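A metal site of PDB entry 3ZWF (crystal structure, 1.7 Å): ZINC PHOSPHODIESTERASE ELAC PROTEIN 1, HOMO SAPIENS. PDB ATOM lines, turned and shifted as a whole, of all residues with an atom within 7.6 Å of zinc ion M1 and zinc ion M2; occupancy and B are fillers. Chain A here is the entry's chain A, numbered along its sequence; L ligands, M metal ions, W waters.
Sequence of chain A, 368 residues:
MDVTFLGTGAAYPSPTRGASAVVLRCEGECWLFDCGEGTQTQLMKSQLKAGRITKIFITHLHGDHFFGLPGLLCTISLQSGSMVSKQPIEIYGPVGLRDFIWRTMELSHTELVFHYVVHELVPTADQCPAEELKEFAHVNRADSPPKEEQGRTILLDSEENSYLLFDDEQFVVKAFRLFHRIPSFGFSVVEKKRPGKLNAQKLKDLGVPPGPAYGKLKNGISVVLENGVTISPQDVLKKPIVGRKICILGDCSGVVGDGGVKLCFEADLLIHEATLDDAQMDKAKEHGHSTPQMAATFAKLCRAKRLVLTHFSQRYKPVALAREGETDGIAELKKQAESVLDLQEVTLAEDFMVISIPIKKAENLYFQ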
ATOM      1  N   GLY A   9      36.972   9.587   0.404  1.00  0.00           N
ATOM      2  CA  GLY A   9      36.826   8.510   1.348  1.00  0.00           C
ATOM      3  C   GLY A   9      35.422   7.979   1.493  1.00  0.00           C
ATOM      4  O   GLY A   9      34.411   8.684   1.233  1.00  0.00           O
ATOM      5  N   ALA A  10      35.352   6.757   2.004  1.00  0.00           N
ATOM      6  CA  ALA A  10      34.092   6.054   2.319  1.00  0.00           C
ATOM      7  C   ALA A  10      33.597   6.318   3.724  1.00  0.00           C
ATOM      8  O   ALA A  10      34.390   6.394   4.640  1.00  0.00           O
ATOM      9  CB  ALA A  10      34.245   4.573   2.166  1.00  0.00           C
ATOM     10  N   ALA A  11      32.279   6.453   3.838  1.00  0.00           N
ATOM     11  CA  ALA A  11      31.517   6.379   5.096  1.00  0.00           C
ATOM     12  C   ALA A  11      31.620   7.563   6.073  1.00  0.00           C
ATOM     13  O   ALA A  11      30.642   7.833   6.785  1.00  0.00           O
ATOM     14  CB  ALA A  11      31.781   5.032   5.808  1.00  0.00           C
ATOM     15  N   TYR A  12      32.766   8.219   6.152  1.00  0.00           N
ATOM     16  CA  TYR A  12      33.001   9.377   6.981  1.00  0.00           C
ATOM     17  C   TYR A  12      34.226  10.120   6.527  1.00  0.00           C
ATOM     18  O   TYR A  12      35.086   9.541   5.859  1.00  0.00           O
ATOM     19  CB  TYR A  12      33.162   8.997   8.466  1.00  0.00           C
ATOM     20  CG  TYR A  12      34.210   7.989   8.742  1.00  0.00           C
ATOM     21  CD1 TYR A  12      33.937   6.625   8.702  1.00  0.00           C
ATOM     22  CD2 TYR A  12      35.518   8.394   9.040  1.00  0.00           C
ATOM     23  CE1 TYR A  12      34.907   5.721   9.000  1.00  0.00           C
ATOM     24  CE2 TYR A  12      36.476   7.498   9.308  1.00  0.00           C
ATOM     25  CZ  TYR A  12      36.182   6.161   9.294  1.00  0.00           C
ATOM     26  OH  TYR A  12      37.191   5.259   9.570  1.00  0.00           O
ATOM     27  N   SER A  20      32.493  12.202   0.692  1.00  0.00           N
ATOM     28  CA  SER A  20      32.198  12.336  -0.749  1.00  0.00           C
ATOM     29  C   SER A  20      31.834  13.753  -1.196  1.00  0.00           C
ATOM     30  O   SER A  20      30.916  14.379  -0.687  1.00  0.00           O
ATOM     31  CB  SER A  20      31.101  11.358  -1.143  1.00  0.00           C
ATOM     32  OG  SER A  20      31.687  10.065  -1.114  1.00  0.00           O
ATOM     33  N   ASP A  34      27.533  15.420  -4.561  1.00  0.00           N
ATOM     34  CA  ASP A  34      27.623  15.026  -3.142  1.00  0.00           C
ATOM     35  C   ASP A  34      28.283  16.085  -2.268  1.00  0.00           C
ATOM     36  O   ASP A  34      29.014  16.969  -2.723  1.00  0.00           O
ATOM     37  CB  ASP A  34      28.219  13.620  -2.959  1.00  0.00           C
ATOM     38  CG  ASP A  34      27.218  12.487  -3.379  1.00  0.00           C
ATOM     39  OD1 ASP A  34      26.048  12.773  -3.463  1.00  0.00           O
ATOM     40  OD2 ASP A  34      27.636  11.327  -3.566  1.00  0.00           O
ATOM     41  N   THR A  59      23.608  11.968  -4.452  1.00  0.00           N
ATOM     42  CA  THR A  59      23.404  10.586  -4.981  1.00  0.00           C
ATOM     43  C   THR A  59      22.502   9.740  -4.086  1.00  0.00           C
ATOM     44  O   THR A  59      21.725   8.943  -4.566  1.00  0.00           O
ATOM     45  CB  THR A  59      24.689   9.832  -5.154  1.00  0.00           C
ATOM     46  OG1 THR A  59      25.403   9.768  -3.905  1.00  0.00           O
ATOM     47  CG2 THR A  59      25.594  10.495  -6.230  1.00  0.00           C
ATOM     48  N   HIS A  60      22.566   9.961  -2.762  1.00  0.00           N
ATOM     49  CA  HIS A  60      21.780   9.192  -1.809  1.00  0.00           C
ATOM     50  C   HIS A  60      21.861   9.830  -0.437  1.00  0.00           C
ATOM     51  O   HIS A  60      22.820  10.528  -0.168  1.00  0.00           O
ATOM     52  CB  HIS A  60      22.162   7.725  -1.767  1.00  0.00           C
ATOM     53  CG  HIS A  60      23.519   7.408  -1.216  1.00  0.00           C
ATOM     54  ND1 HIS A  60      24.718   7.754  -1.833  1.00  0.00           N
ATOM     55  CD2 HIS A  60      23.856   6.571  -0.209  1.00  0.00           C
ATOM     56  CE1 HIS A  60      25.716   7.248  -1.143  1.00  0.00           C
ATOM     57  NE2 HIS A  60      25.233   6.523  -0.149  1.00  0.00           N
ATOM     58  N   LEU A  61      20.872   9.503   0.378  1.00  0.00           N
ATOM     59  CA  LEU A  61      20.776  10.104   1.714  1.00  0.00           C
ATOM     60  C   LEU A  61      21.501   9.304   2.796  1.00  0.00           C
ATOM     61  O   LEU A  61      20.898   8.986   3.842  1.00  0.00           O
ATOM     62  CB  LEU A  61      19.285  10.326   2.057  1.00  0.00           C
ATOM     63  CG  LEU A  61      18.554  11.301   1.129  1.00  0.00           C
ATOM     64  CD1 LEU A  61      17.087  11.511   1.522  1.00  0.00           C
ATOM     65  CD2 LEU A  61      19.310  12.643   1.110  1.00  0.00           C
ATOM     66  N   HIS A  62      22.788   9.038   2.574  1.00  0.00           N
ATOM     67  CA  HIS A  62      23.720   8.619   3.630  1.00  0.00           C
ATOM     68  C   HIS A  62      24.500   9.831   4.021  1.00  0.00           C
ATOM     69  O   HIS A  62      24.826  10.652   3.190  1.00  0.00           O
ATOM     70  CB  HIS A  62      24.636   7.495   3.188  1.00  0.00           C
ATOM     71  CG  HIS A  62      24.016   6.150   3.334  1.00  0.00           C
ATOM     72  ND1 HIS A  62      24.480   5.061   2.638  1.00  0.00           N
ATOM     73  CD2 HIS A  62      23.016   5.697   4.125  1.00  0.00           C
ATOM     74  CE1 HIS A  62      23.791   3.995   2.994  1.00  0.00           C
ATOM     75  NE2 HIS A  62      22.876   4.369   3.890  1.00  0.00           N
ATOM     76  N   GLY A  63      24.794   9.991   5.316  1.00  0.00           N
ATOM     77  CA  GLY A  63      25.342  11.231   5.796  1.00  0.00           C
ATOM     78  C   GLY A  63      26.654  11.702   5.193  1.00  0.00           C
ATOM     79  O   GLY A  63      26.884  12.916   5.059  1.00  0.00           O
ATOM     80  N   ASP A  64      27.500  10.759   4.781  1.00  0.00           N
ATOM     81  CA  ASP A  64      28.777  11.046   4.145  1.00  0.00           C
ATOM     82  C   ASP A  64      28.636  11.622   2.723  1.00  0.00           C
ATOM     83  O   ASP A  64      29.639  11.967   2.101  1.00  0.00           O
ATOM     84  CB  ASP A  64      29.748   9.810   4.087  1.00  0.00           C
ATOM     85  CG  ASP A  64      29.133   8.578   3.541  1.00  0.00           C
ATOM     86  OD1 ASP A  64      27.991   8.181   3.926  1.00  0.00           O
ATOM     87  OD2 ASP A  64      29.824   7.970   2.694  1.00  0.00           O
ATOM     88  N   HIS A  65      27.378  11.734   2.277  1.00  0.00           N
ATOM     89  CA  HIS A  65      27.070  12.371   1.000  1.00  0.00           C
ATOM     90  C   HIS A  65      26.213  13.635   1.098  1.00  0.00           C
ATOM     91  O   HIS A  65      25.949  14.267   0.059  1.00  0.00           O
ATOM     92  CB  HIS A  65      26.432  11.309   0.056  1.00  0.00           C
ATOM     93  CG  HIS A  65      27.308  10.112  -0.107  1.00  0.00           C
ATOM     94  ND1 HIS A  65      28.054   9.877  -1.250  1.00  0.00           N
ATOM     95  CD2 HIS A  65      27.604   9.116   0.742  1.00  0.00           C
ATOM     96  CE1 HIS A  65      28.762   8.785  -1.073  1.00  0.00           C
ATOM     97  NE2 HIS A  65      28.512   8.311   0.134  1.00  0.00           N
ATOM     98  N   HIS A 180      21.788   0.027  -3.645  1.00  0.00           N
ATOM     99  CA  HIS A 180      22.612   0.267  -2.489  1.00  0.00           C
ATOM    100  C   HIS A 180      21.809  -0.123  -1.236  1.00  0.00           C
ATOM    101  O   HIS A 180      20.674  -0.620  -1.352  1.00  0.00           O
ATOM    102  CB  HIS A 180      23.073   1.728  -2.528  1.00  0.00           C
ATOM    103  CG  HIS A 180      24.060   2.130  -1.450  1.00  0.00           C
ATOM    104  ND1 HIS A 180      25.196   1.408  -1.139  1.00  0.00           N
ATOM    105  CD2 HIS A 180      24.060   3.215  -0.644  1.00  0.00           C
ATOM    106  CE1 HIS A 180      25.832   2.032  -0.151  1.00  0.00           C
ATOM    107  NE2 HIS A 180      25.176   3.133   0.158  1.00  0.00           N
ATOM    108  N   ARG A 181      22.353   0.093  -0.042  1.00  0.00           N
ATOM    109  CA  ARG A 181      21.633  -0.196   1.200  1.00  0.00           C
ATOM    110  C   ARG A 181      20.376   0.654   1.335  1.00  0.00           C
ATOM    111  O   ARG A 181      19.364   0.243   1.909  1.00  0.00           O
ATOM    112  CB  ARG A 181      22.541   0.049   2.453  1.00  0.00           C
ATOM    113  CG  ARG A 181      23.758  -0.793   2.516  1.00  0.00           C
ATOM    114  CD  ARG A 181      24.356  -0.855   3.946  1.00  0.00           C
ATOM    115  NE  ARG A 181      24.586   0.448   4.603  1.00  0.00           N
ATOM    116  CZ  ARG A 181      25.464   1.370   4.195  1.00  0.00           C
ATOM    117  NH1 ARG A 181      26.200   1.215   3.085  1.00  0.00           N
ATOM    118  NH2 ARG A 181      25.585   2.490   4.897  1.00  0.00           N
ATOM    119  N   ILE A 182      20.451   1.872   0.787  1.00  0.00           N
ATOM    120  CA  ILE A 182      19.263   2.726   0.583  1.00  0.00           C
ATOM    121  C   ILE A 182      19.318   3.098  -0.890  1.00  0.00           C
ATOM    122  O   ILE A 182      20.356   2.876  -1.528  1.00  0.00           O
ATOM    123  CB  ILE A 182      19.239   3.983   1.472  1.00  0.00           C
ATOM    124  CG1 ILE A 182      20.405   4.921   1.228  1.00  0.00           C
ATOM    125  CG2 ILE A 182      19.152   3.559   2.950  1.00  0.00           C
ATOM    126  CD1 ILE A 182      20.240   6.255   1.882  1.00  0.00           C
ATOM    127  N   SER A 184      20.059   4.749  -4.304  1.00  0.00           N
ATOM    128  CA  SER A 184      21.142   5.579  -4.714  1.00  0.00           C
ATOM    129  C   SER A 184      21.068   5.807  -6.224  1.00  0.00           C
ATOM    130  O   SER A 184      20.470   5.005  -6.955  1.00  0.00           O
ATOM    131  CB  SER A 184      22.469   4.915  -4.287  1.00  0.00           C
ATOM    132  OG  SER A 184      23.627   5.658  -4.685  1.00  0.00           O
ATOM    133  N   GLY A 250      26.764   7.253  -7.531  1.00  0.00           N
ATOM    134  CA  GLY A 250      26.737   7.100  -6.061  1.00  0.00           C
ATOM    135  C   GLY A 250      27.148   5.704  -5.613  1.00  0.00           C
ATOM    136  O   GLY A 250      27.368   4.776  -6.430  1.00  0.00           O
ATOM    137  N   ASP A 251      27.248   5.541  -4.295  1.00  0.00           N
ATOM    138  CA  ASP A 251      27.530   4.234  -3.686  1.00  0.00           C
ATOM    139  C   ASP A 251      26.569   3.217  -4.270  1.00  0.00           C
ATOM    140  O   ASP A 251      25.380   3.464  -4.444  1.00  0.00           O
ATOM    141  CB  ASP A 251      27.282   4.228  -2.198  1.00  0.00           C
ATOM    142  CG  ASP A 251      28.207   5.173  -1.403  1.00  0.00           C
ATOM    143  OD1 ASP A 251      29.050   5.880  -1.977  1.00  0.00           O
ATOM    144  OD2 ASP A 251      28.032   5.236  -0.160  1.00  0.00           O
ATOM    145  N   CYS A 252      27.108   2.047  -4.563  1.00  0.00           N
ATOM    146  CA  CYS A 252      26.314   0.969  -5.187  1.00  0.00           C
ATOM    147  C   CYS A 252      27.095  -0.339  -5.231  1.00  0.00           C
ATOM    148  O   CYS A 252      28.310  -0.353  -5.213  1.00  0.00           O
ATOM    149  CB  CYS A 252      25.912   1.348  -6.609  1.00  0.00           C
ATOM    150  SG  CYS A 252      27.207   1.476  -7.814  1.00  0.00           S
ATOM    151  N   GLU A 273      32.522   4.174  -7.282  1.00  0.00           N
ATOM    152  CA  GLU A 273      33.130   3.725  -6.008  1.00  0.00           C
ATOM    153  C   GLU A 273      33.890   2.391  -6.101  1.00  0.00           C
ATOM    154  O   GLU A 273      33.650   1.533  -6.936  1.00  0.00           O
ATOM    155  CB  GLU A 273      32.077   3.582  -4.921  1.00  0.00           C
ATOM    156  CG  GLU A 273      31.087   2.449  -5.135  1.00  0.00           C
ATOM    157  CD  GLU A 273      30.812   1.766  -3.816  1.00  0.00           C
ATOM    158  OE1 GLU A 273      31.729   1.074  -3.299  1.00  0.00           O
ATOM    159  OE2 GLU A 273      29.724   1.983  -3.250  1.00  0.00           O
ATOM    160  N   THR A 275      34.869   0.734  -2.688  1.00  0.00           N
ATOM    161  CA  THR A 275      35.018   0.858  -1.233  1.00  0.00           C
ATOM    162  C   THR A 275      36.053  -0.121  -0.644  1.00  0.00           C
ATOM    163  O   THR A 275      36.905   0.261   0.181  1.00  0.00           O
ATOM    164  CB  THR A 275      33.672   0.757  -0.472  1.00  0.00           C
ATOM    165  OG1 THR A 275      32.779   1.768  -0.960  1.00  0.00           O
ATOM    166  CG2 THR A 275      33.905   0.915   1.026  1.00  0.00           C
ATOM    167  N   HIS A 287      27.213  -4.659   2.051  1.00  0.00           N
ATOM    168  CA  HIS A 287      27.012  -3.251   2.403  1.00  0.00           C
ATOM    169  C   HIS A 287      26.610  -2.358   1.243  1.00  0.00           C
ATOM    170  O   HIS A 287      26.644  -1.130   1.374  1.00  0.00           O
ATOM    171  CB  HIS A 287      28.252  -2.687   3.084  1.00  0.00           C
ATOM    172  CG  HIS A 287      28.472  -3.252   4.446  1.00  0.00           C
ATOM    173  ND1 HIS A 287      29.267  -4.352   4.677  1.00  0.00           N
ATOM    174  CD2 HIS A 287      27.967  -2.895   5.649  1.00  0.00           C
ATOM    175  CE1 HIS A 287      29.265  -4.633   5.962  1.00  0.00           C
ATOM    176  NE2 HIS A 287      28.473  -3.773   6.581  1.00  0.00           N
ATOM    177  N   GLY A 288      26.221  -2.966   0.121  1.00  0.00           N
ATOM    178  CA  GLY A 288      25.796  -2.204  -1.067  1.00  0.00           C
ATOM    179  C   GLY A 288      26.918  -1.443  -1.754  1.00  0.00           C
ATOM    180  O   GLY A 288      26.716  -0.375  -2.356  1.00  0.00           O
ATOM    181  N   HIS A 289      28.122  -2.030  -1.676  1.00  0.00           N
ATOM    182  CA  HIS A 289      29.325  -1.430  -2.221  1.00  0.00           C
ATOM    183  C   HIS A 289      29.908  -2.288  -3.369  1.00  0.00           C
ATOM    184  O   HIS A 289      29.476  -3.407  -3.597  1.00  0.00           O
ATOM    185  CB  HIS A 289      30.364  -1.174  -1.119  1.00  0.00           C
ATOM    186  CG  HIS A 289      29.993  -0.044  -0.205  1.00  0.00           C
ATOM    187  ND1 HIS A 289      29.606   1.190  -0.674  1.00  0.00           N
ATOM    188  CD2 HIS A 289      29.981   0.051   1.150  1.00  0.00           C
ATOM    189  CE1 HIS A 289      29.338   1.994   0.348  1.00  0.00           C
ATOM    190  NE2 HIS A 289      29.527   1.311   1.472  1.00  0.00           N
ATOM    191  N   HIS A 311      35.798   6.832  -3.192  1.00  0.00           N
ATOM    192  CA  HIS A 311      35.063   6.288  -2.034  1.00  0.00           C
ATOM    193  C   HIS A 311      35.744   5.074  -1.457  1.00  0.00           C
ATOM    194  O   HIS A 311      35.128   4.060  -1.208  1.00  0.00           O
ATOM    195  CB  HIS A 311      33.594   5.977  -2.398  1.00  0.00           C
ATOM    196  CG  HIS A 311      32.661   5.827  -1.232  1.00  0.00           C
ATOM    197  ND1 HIS A 311      32.398   4.618  -0.626  1.00  0.00           N
ATOM    198  CD2 HIS A 311      31.819   6.718  -0.665  1.00  0.00           C
ATOM    199  CE1 HIS A 311      31.493   4.781   0.325  1.00  0.00           C
ATOM    200  NE2 HIS A 311      31.097   6.044   0.295  1.00  0.00           N
HETATM  201  P1  LIG L   1      28.658   3.946   3.220  1.00  0.00           P
HETATM  202  O1  LIG L   1      27.413   3.577   2.360  1.00  0.00           O
HETATM  203  O2  LIG L   1      28.026   4.705   4.506  1.00  0.00           O
HETATM  204  O3  LIG L   1      29.482   4.977   2.562  1.00  0.00           O
HETATM  205  O4  LIG L   1      29.261   2.672   3.671  1.00  0.00           O
HETATM  206 ZN    ZN M   1      26.125   4.917   1.234  1.00  0.00          ZN
HETATM  207 ZN    ZN M   2      29.164   6.509   1.208  1.00  0.00          ZN
HETATM  208  O   HOH W   1      27.227   6.390   2.175  1.00  0.00           O
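The nearest printed residue that does not touch zinc ion M2 is Ala 11 (4.1 Å).
NE2 of His 62 lies close to NH2 of Arg 181 (3.4 Å).
The side-chain carboxylate of Asp 64 lies close to the backbone NH of Ala 11 (3.1 Å).
N of Ser 20 sits at hydrogen-bond distance from O of Asp 64.
O of Asp 251 is in hydrogen-bond range of OG of Ser 184 (2.8 Å).
OG1 of Thr 275 lies within hydrogen-bond range of ND1 of His 311, 2.9 Å away.
A ring nitrogen (ND1) of His 65 is in hydrogen-bond range of the side-chain carboxylate (OD2) of Asp 34, at 2.8 Å.
A ring nitrogen (ND1) of His 180 lies within hydrogen-bond range of the backbone carbonyl oxygen (O) of Gly 288.
ND1 of His 60 sits at hydrogen-bond distance from OG1 of Thr 59 (3.0 Å).
Of the 26 residues printed, 4 come within 4 Å of zinc ion M1.
Along chain A the residues within 4 Å of zinc ion M1 span positions 60 to 251.
Zinc ion M2 is bound by O3 of the ligand (2.1 Å).
Water W1 is bound to zinc ion M2 (2.2 Å).
Zinc ion M2 is bound by the side-chain carboxylate (OD2) of Asp 64 (2.2 Å).
Zinc ion M2 is bound by the side-chain carboxylate (OD2) of Asp 251.
NE2 of His 311 is bound to zinc ion M2.
NE2 of His 65 binds zinc ion M2, 2.2 Å away.
Zinc ion M1 is bound by water W1 (2.1 Å), a ring nitrogen (ND1) of His 62 (2.2 Å), an oxygen (O1) of the ligand (2.2 Å), a ring nitrogen (NE2) of His 180 (2.3 Å), a ring nitrogen (NE2) of His 60 (2.3 Å) and the side-chain carboxylate (OD2) of Asp 251 (2.4 Å).
Zinc ion M1 has six donor atoms within binding distance.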
